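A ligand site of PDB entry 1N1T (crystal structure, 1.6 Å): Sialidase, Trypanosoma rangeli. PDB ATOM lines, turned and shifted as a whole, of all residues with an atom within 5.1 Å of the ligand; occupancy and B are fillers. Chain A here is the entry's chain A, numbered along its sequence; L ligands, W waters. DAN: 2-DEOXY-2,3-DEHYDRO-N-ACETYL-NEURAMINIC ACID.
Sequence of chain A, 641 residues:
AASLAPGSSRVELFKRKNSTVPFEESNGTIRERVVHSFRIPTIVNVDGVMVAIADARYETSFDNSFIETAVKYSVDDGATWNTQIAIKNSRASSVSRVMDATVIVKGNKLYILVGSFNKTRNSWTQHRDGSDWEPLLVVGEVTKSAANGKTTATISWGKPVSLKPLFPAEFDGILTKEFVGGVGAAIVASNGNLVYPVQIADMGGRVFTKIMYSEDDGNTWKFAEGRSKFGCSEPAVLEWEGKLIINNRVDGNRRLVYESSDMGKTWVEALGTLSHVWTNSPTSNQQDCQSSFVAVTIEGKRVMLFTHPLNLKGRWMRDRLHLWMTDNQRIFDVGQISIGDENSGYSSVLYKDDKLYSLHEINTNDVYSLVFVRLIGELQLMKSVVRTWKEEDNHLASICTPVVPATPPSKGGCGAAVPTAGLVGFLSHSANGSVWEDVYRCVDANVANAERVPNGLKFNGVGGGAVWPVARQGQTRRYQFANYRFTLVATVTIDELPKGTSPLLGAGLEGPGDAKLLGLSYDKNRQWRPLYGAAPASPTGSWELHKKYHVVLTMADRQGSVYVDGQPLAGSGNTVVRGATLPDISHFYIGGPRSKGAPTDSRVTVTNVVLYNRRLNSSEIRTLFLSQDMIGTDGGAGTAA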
ATOM      1  N   ARG A  39     -12.024   5.513  12.172  1.00  0.00           N
ATOM      2  CA  ARG A  39     -11.372   6.155  13.314  1.00  0.00           C
ATOM      3  C   ARG A  39     -12.010   7.492  13.641  1.00  0.00           C
ATOM      4  O   ARG A  39     -12.888   7.983  12.920  1.00  0.00           O
ATOM      5  CB  ARG A  39      -9.888   6.401  13.020  1.00  0.00           C
ATOM      6  CG  ARG A  39      -9.020   5.108  13.053  1.00  0.00           C
ATOM      7  CD  ARG A  39      -7.556   5.359  13.401  1.00  0.00           C
ATOM      8  NE  ARG A  39      -7.503   6.008  14.697  1.00  0.00           N
ATOM      9  CZ  ARG A  39      -6.545   6.773  15.168  1.00  0.00           C
ATOM     10  NH1 ARG A  39      -6.723   7.338  16.347  1.00  0.00           N
ATOM     11  NH2 ARG A  39      -5.442   7.012  14.480  1.00  0.00           N
ATOM     12  N   ILE A  40     -11.576   8.039  14.758  1.00  0.00           N
ATOM     13  CA  ILE A  40     -11.940   9.404  15.160  1.00  0.00           C
ATOM     14  C   ILE A  40     -13.459   9.588  15.343  1.00  0.00           C
ATOM     15  O   ILE A  40     -14.095  10.392  14.633  1.00  0.00           O
ATOM     16  CB  ILE A  40     -11.389  10.434  14.131  1.00  0.00           C
ATOM     17  CG1 ILE A  40     -10.021  10.040  13.540  1.00  0.00           C
ATOM     18  CG2 ILE A  40     -11.252  11.793  14.805  1.00  0.00           C
ATOM     19  CD1 ILE A  40      -8.876   9.844  14.530  1.00  0.00           C
ATOM     20  N   ASP A  55     -13.948   9.145  10.696  1.00  0.00           N
ATOM     21  CA  ASP A  55     -13.074   9.090   9.536  1.00  0.00           C
ATOM     22  C   ASP A  55     -13.309   7.706   8.908  1.00  0.00           C
ATOM     23  O   ASP A  55     -13.174   6.675   9.593  1.00  0.00           O
ATOM     24  CB  ASP A  55     -11.611   9.007   9.949  1.00  0.00           C
ATOM     25  CG  ASP A  55     -10.896  10.327  10.061  1.00  0.00           C
ATOM     26  OD1 ASP A  55     -11.518  11.407  10.221  1.00  0.00           O
ATOM     27  OD2 ASP A  55      -9.631  10.342  10.014  1.00  0.00           O
ATOM     28  N   ARG A  57     -11.331   5.467   6.755  1.00  0.00           N
ATOM     29  CA  ARG A  57      -9.978   5.365   6.209  1.00  0.00           C
ATOM     30  C   ARG A  57     -10.027   4.157   5.287  1.00  0.00           C
ATOM     31  O   ARG A  57      -9.881   3.007   5.712  1.00  0.00           O
ATOM     32  CB  ARG A  57      -8.926   5.228   7.303  1.00  0.00           C
ATOM     33  CG  ARG A  57      -9.048   6.383   8.311  1.00  0.00           C
ATOM     34  CD  ARG A  57      -7.821   6.579   9.155  1.00  0.00           C
ATOM     35  NE  ARG A  57      -7.916   7.838   9.932  1.00  0.00           N
ATOM     36  CZ  ARG A  57      -6.936   8.377  10.651  1.00  0.00           C
ATOM     37  NH1 ARG A  57      -5.759   7.754  10.775  1.00  0.00           N
ATOM     38  NH2 ARG A  57      -7.125   9.571  11.277  1.00  0.00           N
ATOM     39  N   ASP A  63      -2.573   7.904   8.979  1.00  0.00           N
ATOM     40  CA  ASP A  63      -3.152   9.252   8.914  1.00  0.00           C
ATOM     41  C   ASP A  63      -3.084   9.820   7.519  1.00  0.00           C
ATOM     42  O   ASP A  63      -3.996  10.474   7.057  1.00  0.00           O
ATOM     43  CB  ASP A  63      -2.369  10.199   9.805  1.00  0.00           C
ATOM     44  CG  ASP A  63      -2.514   9.865  11.264  1.00  0.00           C
ATOM     45  OD1 ASP A  63      -1.642  10.345  12.052  1.00  0.00           O
ATOM     46  OD2 ASP A  63      -3.450   9.183  11.726  1.00  0.00           O
ATOM     47  N   ASN A  64      -1.983   9.566   6.831  1.00  0.00           N
ATOM     48  CA  ASN A  64      -1.806  10.191   5.532  1.00  0.00           C
ATOM     49  C   ASN A  64      -2.160   9.222   4.427  1.00  0.00           C
ATOM     50  O   ASN A  64      -1.297   8.675   3.719  1.00  0.00           O
ATOM     51  CB  ASN A  64      -0.404  10.778   5.473  1.00  0.00           C
ATOM     52  CG  ASN A  64      -0.075  11.523   6.764  1.00  0.00           C
ATOM     53  OD1 ASN A  64      -0.842  12.407   7.247  1.00  0.00           O
ATOM     54  ND2 ASN A  64       0.992  11.099   7.406  1.00  0.00           N
ATOM     55  N   MET A  99     -10.195  14.955   7.427  1.00  0.00           N
ATOM     56  CA  MET A  99     -10.022  14.187   8.665  1.00  0.00           C
ATOM     57  C   MET A  99     -10.168  14.987   9.957  1.00  0.00           C
ATOM     58  O   MET A  99     -10.249  16.207   9.937  1.00  0.00           O
ATOM     59  CB  MET A  99      -8.665  13.506   8.613  1.00  0.00           C
ATOM     60  CG  MET A  99      -7.494  14.527   8.705  1.00  0.00           C
ATOM     61  SD  MET A  99      -5.843  13.871   8.157  1.00  0.00           S
ATOM     62  CE  MET A  99      -5.566  12.546   9.430  1.00  0.00           C
ATOM     63  N   ASP A 100     -10.254  14.247  11.063  1.00  0.00           N
ATOM     64  CA  ASP A 100     -10.285  14.813  12.403  1.00  0.00           C
ATOM     65  C   ASP A 100     -11.493  15.727  12.647  1.00  0.00           C
ATOM     66  O   ASP A 100     -11.363  16.861  13.130  1.00  0.00           O
ATOM     67  CB  ASP A 100      -8.969  15.537  12.669  1.00  0.00           C
ATOM     68  CG  ASP A 100      -7.811  14.586  12.895  1.00  0.00           C
ATOM     69  OD1 ASP A 100      -7.964  13.371  12.610  1.00  0.00           O
ATOM     70  OD2 ASP A 100      -6.714  14.985  13.343  1.00  0.00           O
ATOM     71  N   PHE A 117      -6.485  17.698   3.158  1.00  0.00           N
ATOM     72  CA  PHE A 117      -5.120  17.666   2.607  1.00  0.00           C
ATOM     73  C   PHE A 117      -5.170  17.035   1.231  1.00  0.00           C
ATOM     74  O   PHE A 117      -5.980  16.163   0.969  1.00  0.00           O
ATOM     75  CB  PHE A 117      -4.254  16.848   3.559  1.00  0.00           C
ATOM     76  CG  PHE A 117      -4.139  17.453   4.914  1.00  0.00           C
ATOM     77  CD1 PHE A 117      -5.043  17.090   5.917  1.00  0.00           C
ATOM     78  CD2 PHE A 117      -3.140  18.387   5.215  1.00  0.00           C
ATOM     79  CE1 PHE A 117      -4.958  17.650   7.194  1.00  0.00           C
ATOM     80  CE2 PHE A 117      -3.057  18.937   6.523  1.00  0.00           C
ATOM     81  CZ  PHE A 117      -3.962  18.564   7.504  1.00  0.00           C
ATOM     82  N   SER A 123       3.353  14.120   8.319  1.00  0.00           N
ATOM     83  CA  SER A 123       2.426  14.604   9.360  1.00  0.00           C
ATOM     84  C   SER A 123       2.267  16.109   9.309  1.00  0.00           C
ATOM     85  O   SER A 123       3.233  16.853   9.065  1.00  0.00           O
ATOM     86  CB  SER A 123       2.930  14.143  10.753  1.00  0.00           C
ATOM     87  OG  SER A 123       1.840  14.114  11.692  1.00  0.00           O
ATOM     88  N   TRP A 124       1.052  16.561   9.562  1.00  0.00           N
ATOM     89  CA  TRP A 124       0.695  17.966   9.395  1.00  0.00           C
ATOM     90  C   TRP A 124       1.585  18.981  10.074  1.00  0.00           C
ATOM     91  O   TRP A 124       1.910  20.035   9.488  1.00  0.00           O
ATOM     92  CB  TRP A 124      -0.795  18.164   9.755  1.00  0.00           C
ATOM     93  CG  TRP A 124      -1.124  18.218  11.238  1.00  0.00           C
ATOM     94  CD1 TRP A 124      -1.097  17.165  12.159  1.00  0.00           C
ATOM     95  CD2 TRP A 124      -1.537  19.363  11.971  1.00  0.00           C
ATOM     96  NE1 TRP A 124      -1.478  17.618  13.401  1.00  0.00           N
ATOM     97  CE2 TRP A 124      -1.741  18.959  13.319  1.00  0.00           C
ATOM     98  CE3 TRP A 124      -1.745  20.704  11.623  1.00  0.00           C
ATOM     99  CZ2 TRP A 124      -2.155  19.830  14.304  1.00  0.00           C
ATOM    100  CZ3 TRP A 124      -2.158  21.584  12.631  1.00  0.00           C
ATOM    101  CH2 TRP A 124      -2.361  21.135  13.955  1.00  0.00           C
ATOM    102  N   THR A 125       2.034  18.699  11.289  1.00  0.00           N
ATOM    103  CA  THR A 125       2.857  19.685  11.996  1.00  0.00           C
ATOM    104  C   THR A 125       4.218  19.855  11.349  1.00  0.00           C
ATOM    105  O   THR A 125       4.887  20.834  11.625  1.00  0.00           O
ATOM    106  CB  THR A 125       3.080  19.273  13.471  1.00  0.00           C
ATOM    107  OG1 THR A 125       3.609  17.944  13.502  1.00  0.00           O
ATOM    108  CG2 THR A 125       1.739  19.198  14.191  1.00  0.00           C
ATOM    109  N   GLN A 199      -6.380  23.439  17.269  1.00  0.00           N
ATOM    110  CA  GLN A 199      -4.959  23.173  17.469  1.00  0.00           C
ATOM    111  C   GLN A 199      -4.223  23.803  16.270  1.00  0.00           C
ATOM    112  O   GLN A 199      -4.635  23.656  15.112  1.00  0.00           O
ATOM    113  CB  GLN A 199      -4.693  21.678  17.576  1.00  0.00           C
ATOM    114  CG  GLN A 199      -5.358  20.834  16.520  1.00  0.00           C
ATOM    115  CD  GLN A 199      -5.233  19.344  16.789  1.00  0.00           C
ATOM    116  OE1 GLN A 199      -6.121  18.562  16.431  1.00  0.00           O
ATOM    117  NE2 GLN A 199      -4.155  18.944  17.455  1.00  0.00           N
ATOM    118  N   SER A 233      -2.229  19.837  22.165  1.00  0.00           N
ATOM    119  CA  SER A 233      -2.925  19.529  20.938  1.00  0.00           C
ATOM    120  C   SER A 233      -4.337  18.976  21.256  1.00  0.00           C
ATOM    121  O   SER A 233      -4.730  18.921  22.426  1.00  0.00           O
ATOM    122  CB  SER A 233      -2.123  18.554  20.093  1.00  0.00           C
ATOM    123  OG  SER A 233      -2.088  17.283  20.767  1.00  0.00           O
ATOM    124  N   GLU A 234      -5.097  18.630  20.217  1.00  0.00           N
ATOM    125  CA  GLU A 234      -6.457  18.049  20.327  1.00  0.00           C
ATOM    126  C   GLU A 234      -7.232  18.528  21.541  1.00  0.00           C
ATOM    127  O   GLU A 234      -7.590  17.726  22.404  1.00  0.00           O
ATOM    128  CB  GLU A 234      -6.410  16.508  20.339  1.00  0.00           C
ATOM    129  CG  GLU A 234      -6.171  16.010  18.927  1.00  0.00           C
ATOM    130  CD  GLU A 234      -5.985  14.523  18.799  1.00  0.00           C
ATOM    131  OE1 GLU A 234      -5.825  13.821  19.825  1.00  0.00           O
ATOM    132  OE2 GLU A 234      -5.999  14.066  17.626  1.00  0.00           O
ATOM    133  N   ARG A 249      -4.772  17.535  24.951  1.00  0.00           N
ATOM    134  CA  ARG A 249      -3.843  16.438  24.748  1.00  0.00           C
ATOM    135  C   ARG A 249      -2.411  16.980  24.913  1.00  0.00           C
ATOM    136  O   ARG A 249      -2.077  18.077  24.450  1.00  0.00           O
ATOM    137  CB  ARG A 249      -4.012  15.850  23.342  1.00  0.00           C
ATOM    138  CG  ARG A 249      -3.148  14.657  23.044  1.00  0.00           C
ATOM    139  CD  ARG A 249      -3.376  14.090  21.670  1.00  0.00           C
ATOM    140  NE  ARG A 249      -2.226  13.271  21.260  1.00  0.00           N
ATOM    141  CZ  ARG A 249      -2.262  12.466  20.199  1.00  0.00           C
ATOM    142  NH1 ARG A 249      -3.387  12.294  19.516  1.00  0.00           N
ATOM    143  NH2 ARG A 249      -1.174  11.814  19.846  1.00  0.00           N
ATOM    144  N   ASP A 251       1.294  15.240  24.395  1.00  0.00           N
ATOM    145  CA  ASP A 251       2.132  14.073  24.176  1.00  0.00           C
ATOM    146  C   ASP A 251       3.343  14.170  25.082  1.00  0.00           C
ATOM    147  O   ASP A 251       3.981  15.225  25.159  1.00  0.00           O
ATOM    148  CB  ASP A 251       2.598  14.040  22.730  1.00  0.00           C
ATOM    149  CG  ASP A 251       1.479  13.769  21.774  1.00  0.00           C
ATOM    150  OD1 ASP A 251       1.462  14.410  20.706  1.00  0.00           O
ATOM    151  OD2 ASP A 251       0.605  12.921  22.013  1.00  0.00           O
ATOM    152  N   GLN A 287       3.093   8.825  24.054  1.00  0.00           N
ATOM    153  CA  GLN A 287       2.131   9.509  23.195  1.00  0.00           C
ATOM    154  C   GLN A 287       0.785   9.601  23.943  1.00  0.00           C
ATOM    155  O   GLN A 287       0.347   8.652  24.579  1.00  0.00           O
ATOM    156  CB  GLN A 287       1.964   8.627  21.943  1.00  0.00           C
ATOM    157  CG  GLN A 287       1.049   9.086  20.848  1.00  0.00           C
ATOM    158  CD  GLN A 287       1.115   8.169  19.615  1.00  0.00           C
ATOM    159  OE1 GLN A 287       0.406   8.420  18.631  1.00  0.00           O
ATOM    160  NE2 GLN A 287       1.927   7.123  19.664  1.00  0.00           N
ATOM    161  N   ASP A 288       0.147  10.759  23.871  1.00  0.00           N
ATOM    162  CA  ASP A 288      -1.165  10.912  24.493  1.00  0.00           C
ATOM    163  C   ASP A 288      -2.248  10.566  23.462  1.00  0.00           C
ATOM    164  O   ASP A 288      -1.954  10.031  22.388  1.00  0.00           O
ATOM    165  CB  ASP A 288      -1.270  12.336  25.045  1.00  0.00           C
ATOM    166  CG  ASP A 288      -2.399  12.536  26.034  1.00  0.00           C
ATOM    167  OD1 ASP A 288      -3.054  11.566  26.448  1.00  0.00           O
ATOM    168  OD2 ASP A 288      -2.687  13.696  26.422  1.00  0.00           O
ATOM    169  N   ARG A 318      -3.254   2.282  23.703  1.00  0.00           N
ATOM    170  CA  ARG A 318      -4.468   2.929  24.258  1.00  0.00           C
ATOM    171  C   ARG A 318      -5.476   1.932  24.795  1.00  0.00           C
ATOM    172  O   ARG A 318      -6.688   2.058  24.626  1.00  0.00           O
ATOM    173  CB  ARG A 318      -5.084   3.822  23.190  1.00  0.00           C
ATOM    174  CG  ARG A 318      -4.193   5.022  22.923  1.00  0.00           C
ATOM    175  CD  ARG A 318      -4.446   5.623  21.578  1.00  0.00           C
ATOM    176  NE  ARG A 318      -3.576   6.805  21.382  1.00  0.00           N
ATOM    177  CZ  ARG A 318      -3.505   7.466  20.218  1.00  0.00           C
ATOM    178  NH1 ARG A 318      -4.231   7.078  19.201  1.00  0.00           N
ATOM    179  NH2 ARG A 318      -2.714   8.544  20.079  1.00  0.00           N
ATOM    180  N   TYR A 346      -9.493   6.646  20.544  1.00  0.00           N
ATOM    181  CA  TYR A 346     -10.308   7.844  20.566  1.00  0.00           C
ATOM    182  C   TYR A 346     -11.759   7.478  20.939  1.00  0.00           C
ATOM    183  O   TYR A 346     -12.202   6.346  20.705  1.00  0.00           O
ATOM    184  CB  TYR A 346     -10.283   8.536  19.187  1.00  0.00           C
ATOM    185  CG  TYR A 346      -9.028   9.330  18.864  1.00  0.00           C
ATOM    186  CD1 TYR A 346      -7.755   8.928  19.298  1.00  0.00           C
ATOM    187  CD2 TYR A 346      -9.096  10.465  18.077  1.00  0.00           C
ATOM    188  CE1 TYR A 346      -6.623   9.678  18.980  1.00  0.00           C
ATOM    189  CE2 TYR A 346      -7.957  11.213  17.746  1.00  0.00           C
ATOM    190  CZ  TYR A 346      -6.731  10.793  18.185  1.00  0.00           C
ATOM    191  OH  TYR A 346      -5.614  11.529  17.878  1.00  0.00           O
HETATM  192  C1  DAN L   1      -3.518   9.756  16.717  1.00  0.00           C
HETATM  193  C2  DAN L   1      -3.753  10.747  15.749  1.00  0.00           C
HETATM  194  C3  DAN L   1      -4.961  10.634  14.885  1.00  0.00           C
HETATM  195  C4  DAN L   1      -5.225  11.912  14.088  1.00  0.00           C
HETATM  196  C5  DAN L   1      -3.937  12.630  13.745  1.00  0.00           C
HETATM  197  C6  DAN L   1      -3.199  12.911  15.050  1.00  0.00           C
HETATM  198  C7  DAN L   1      -1.881  13.662  14.857  1.00  0.00           C
HETATM  199  C8  DAN L   1      -1.115  13.805  16.155  1.00  0.00           C
HETATM  200  C9  DAN L   1       0.224  14.521  15.915  1.00  0.00           C
HETATM  201  C10 DAN L   1      -3.590  14.329  12.029  1.00  0.00           C
HETATM  202  C11 DAN L   1      -4.106  15.520  11.255  1.00  0.00           C
HETATM  203  N5  DAN L   1      -4.326  13.813  13.007  1.00  0.00           N
HETATM  204  O1A DAN L   1      -4.146   8.541  16.676  1.00  0.00           O
HETATM  205  O1B DAN L   1      -2.628   9.959  17.625  1.00  0.00           O
HETATM  206  O4  DAN L   1      -5.951  11.552  12.903  1.00  0.00           O
HETATM  207  O6  DAN L   1      -2.883  11.674  15.684  1.00  0.00           O
HETATM  208  O7  DAN L   1      -1.007  12.970  13.963  1.00  0.00           O
HETATM  209  O8  DAN L   1      -1.878  14.583  17.088  1.00  0.00           O
HETATM  210  O9  DAN L   1       0.069  15.834  15.430  1.00  0.00           O
HETATM  211  O10 DAN L   1      -2.361  13.824  11.697  1.00  0.00           O
HETATM  212  O   HOH W   1      -3.173  16.691  15.937  1.00  0.00           O
HETATM  213  O   HOH W   2       1.886  16.113  13.329  1.00  0.00           O
HETATM  214  O   HOH W   3      -0.107  10.352  17.293  1.00  0.00           O
HETATM  215  O   HOH W   4      -0.646  15.483  19.308  1.00  0.00           O
HETATM  216  O   HOH W   5      -1.071  14.430   9.484  1.00  0.00           O
HETATM  217  O   HOH W   6       0.268  17.434  17.448  1.00  0.00           O
HETATM  218  O   HOH W   7      -0.858  10.008  14.388  1.00  0.00           O
HETATM  219  O   HOH W   8      -2.042   6.595  16.393  1.00  0.00           O
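NH2 of Arg 318 is in salt-bridge range of O1B of the ligand, at 2.8 Å. O1B of the ligand lies within salt-bridge range of NH1 of Arg 249 (3.1 Å). O7 of the ligand is in hydrogen-bond range of OD1 of Asp 63 (3.3 Å). NH1 of Arg 39 is in salt-bridge range of O1A of the ligand (2.9 Å). O9 of the ligand lies within hydrogen-bond range of NE1 of Trp 124, at 3.1 Å. The side-chain carboxylate of Asp 100 sits at hydrogen-bond distance from a nitrogen (N5) of the ligand (2.7 Å). NH2 of Arg 57 is in hydrogen-bond range of O4 of the ligand (2.8 Å). An oxygen (O1B) of the ligand lies close to the side-chain hydroxyl (OH) of Tyr 346, at 3.4 Å.
OH of Tyr 346 lies within hydrogen-bond range of NH1 of Arg 249. The side-chain hydroxyl of Tyr 346 sits at hydrogen-bond distance from the side-chain carboxylate of Glu 234. The guanidinium group of Arg 249 is in salt-bridge range of the side-chain carboxylate of Glu 234 (2.9 Å). NE2 of Gln 199 sits close to N of Glu 234, at 2.9 Å. N of Asp 100 sits at hydrogen-bond distance from OD1 of Asp 55, 3.2 Å away. The guanidinium group (NE) of Arg 249 is in salt-bridge range of the side-chain carboxylate (OD2) of Asp 251. The guanidinium group (NH2) of Arg 57 lies within salt-bridge range of the side-chain carboxylate (OD2) of Asp 55, 2.9 Å away. The guanidinium group (NH2) of Arg 318 lies within hydrogen-bond range of the side-chain amide oxygen (OE1) of Gln 287 (3.4 Å).
Merely in contact with the ligand: Gln 287, Met 99, Ile 40, Ser 123, Thr 125 and Glu 234. Hydrophobic or aromatic side chains within 4 Å of the ligand: Ile 40, Met 99, Trp 124 and Tyr 346. Of the 21 residues printed, 14 come within 4 Å of the ligand.
Water W3 lies within hydrogen-bond range of the side-chain amide oxygen of Gln 287 (2.4 Å), an oxygen (O1B) of the ligand (2.6 Å) and the guanidinium group of Arg 249 (3.1 Å). Water W5 lies within hydrogen-bond range of an oxygen (O10) of the ligand, the backbone NH (N) of Trp 124 and the side-chain amide oxygen (OD1) of Asn 64. Water W4 lies within hydrogen-bond range of O8 of the ligand (2.7 Å), OG of Ser 233 (2.7 Å), OD1 of Asp 251 (2.7 Å) and NE of Arg 249 (3.3 Å). Water W1 lies within hydrogen-bond range of an oxygen (O8) of the ligand, the side-chain amide nitrogen of Gln 199 and the indole nitrogen of Trp 124. Water W2 lies within hydrogen-bond range of OG1 of Thr 125 (2.5 Å), OG of Ser 123 (2.6 Å) and O9 of the ligand (2.8 Å). Water W7 lies within hydrogen-bond range of the side-chain carboxylate of Asp 63 and an oxygen (O6) of the ligand.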
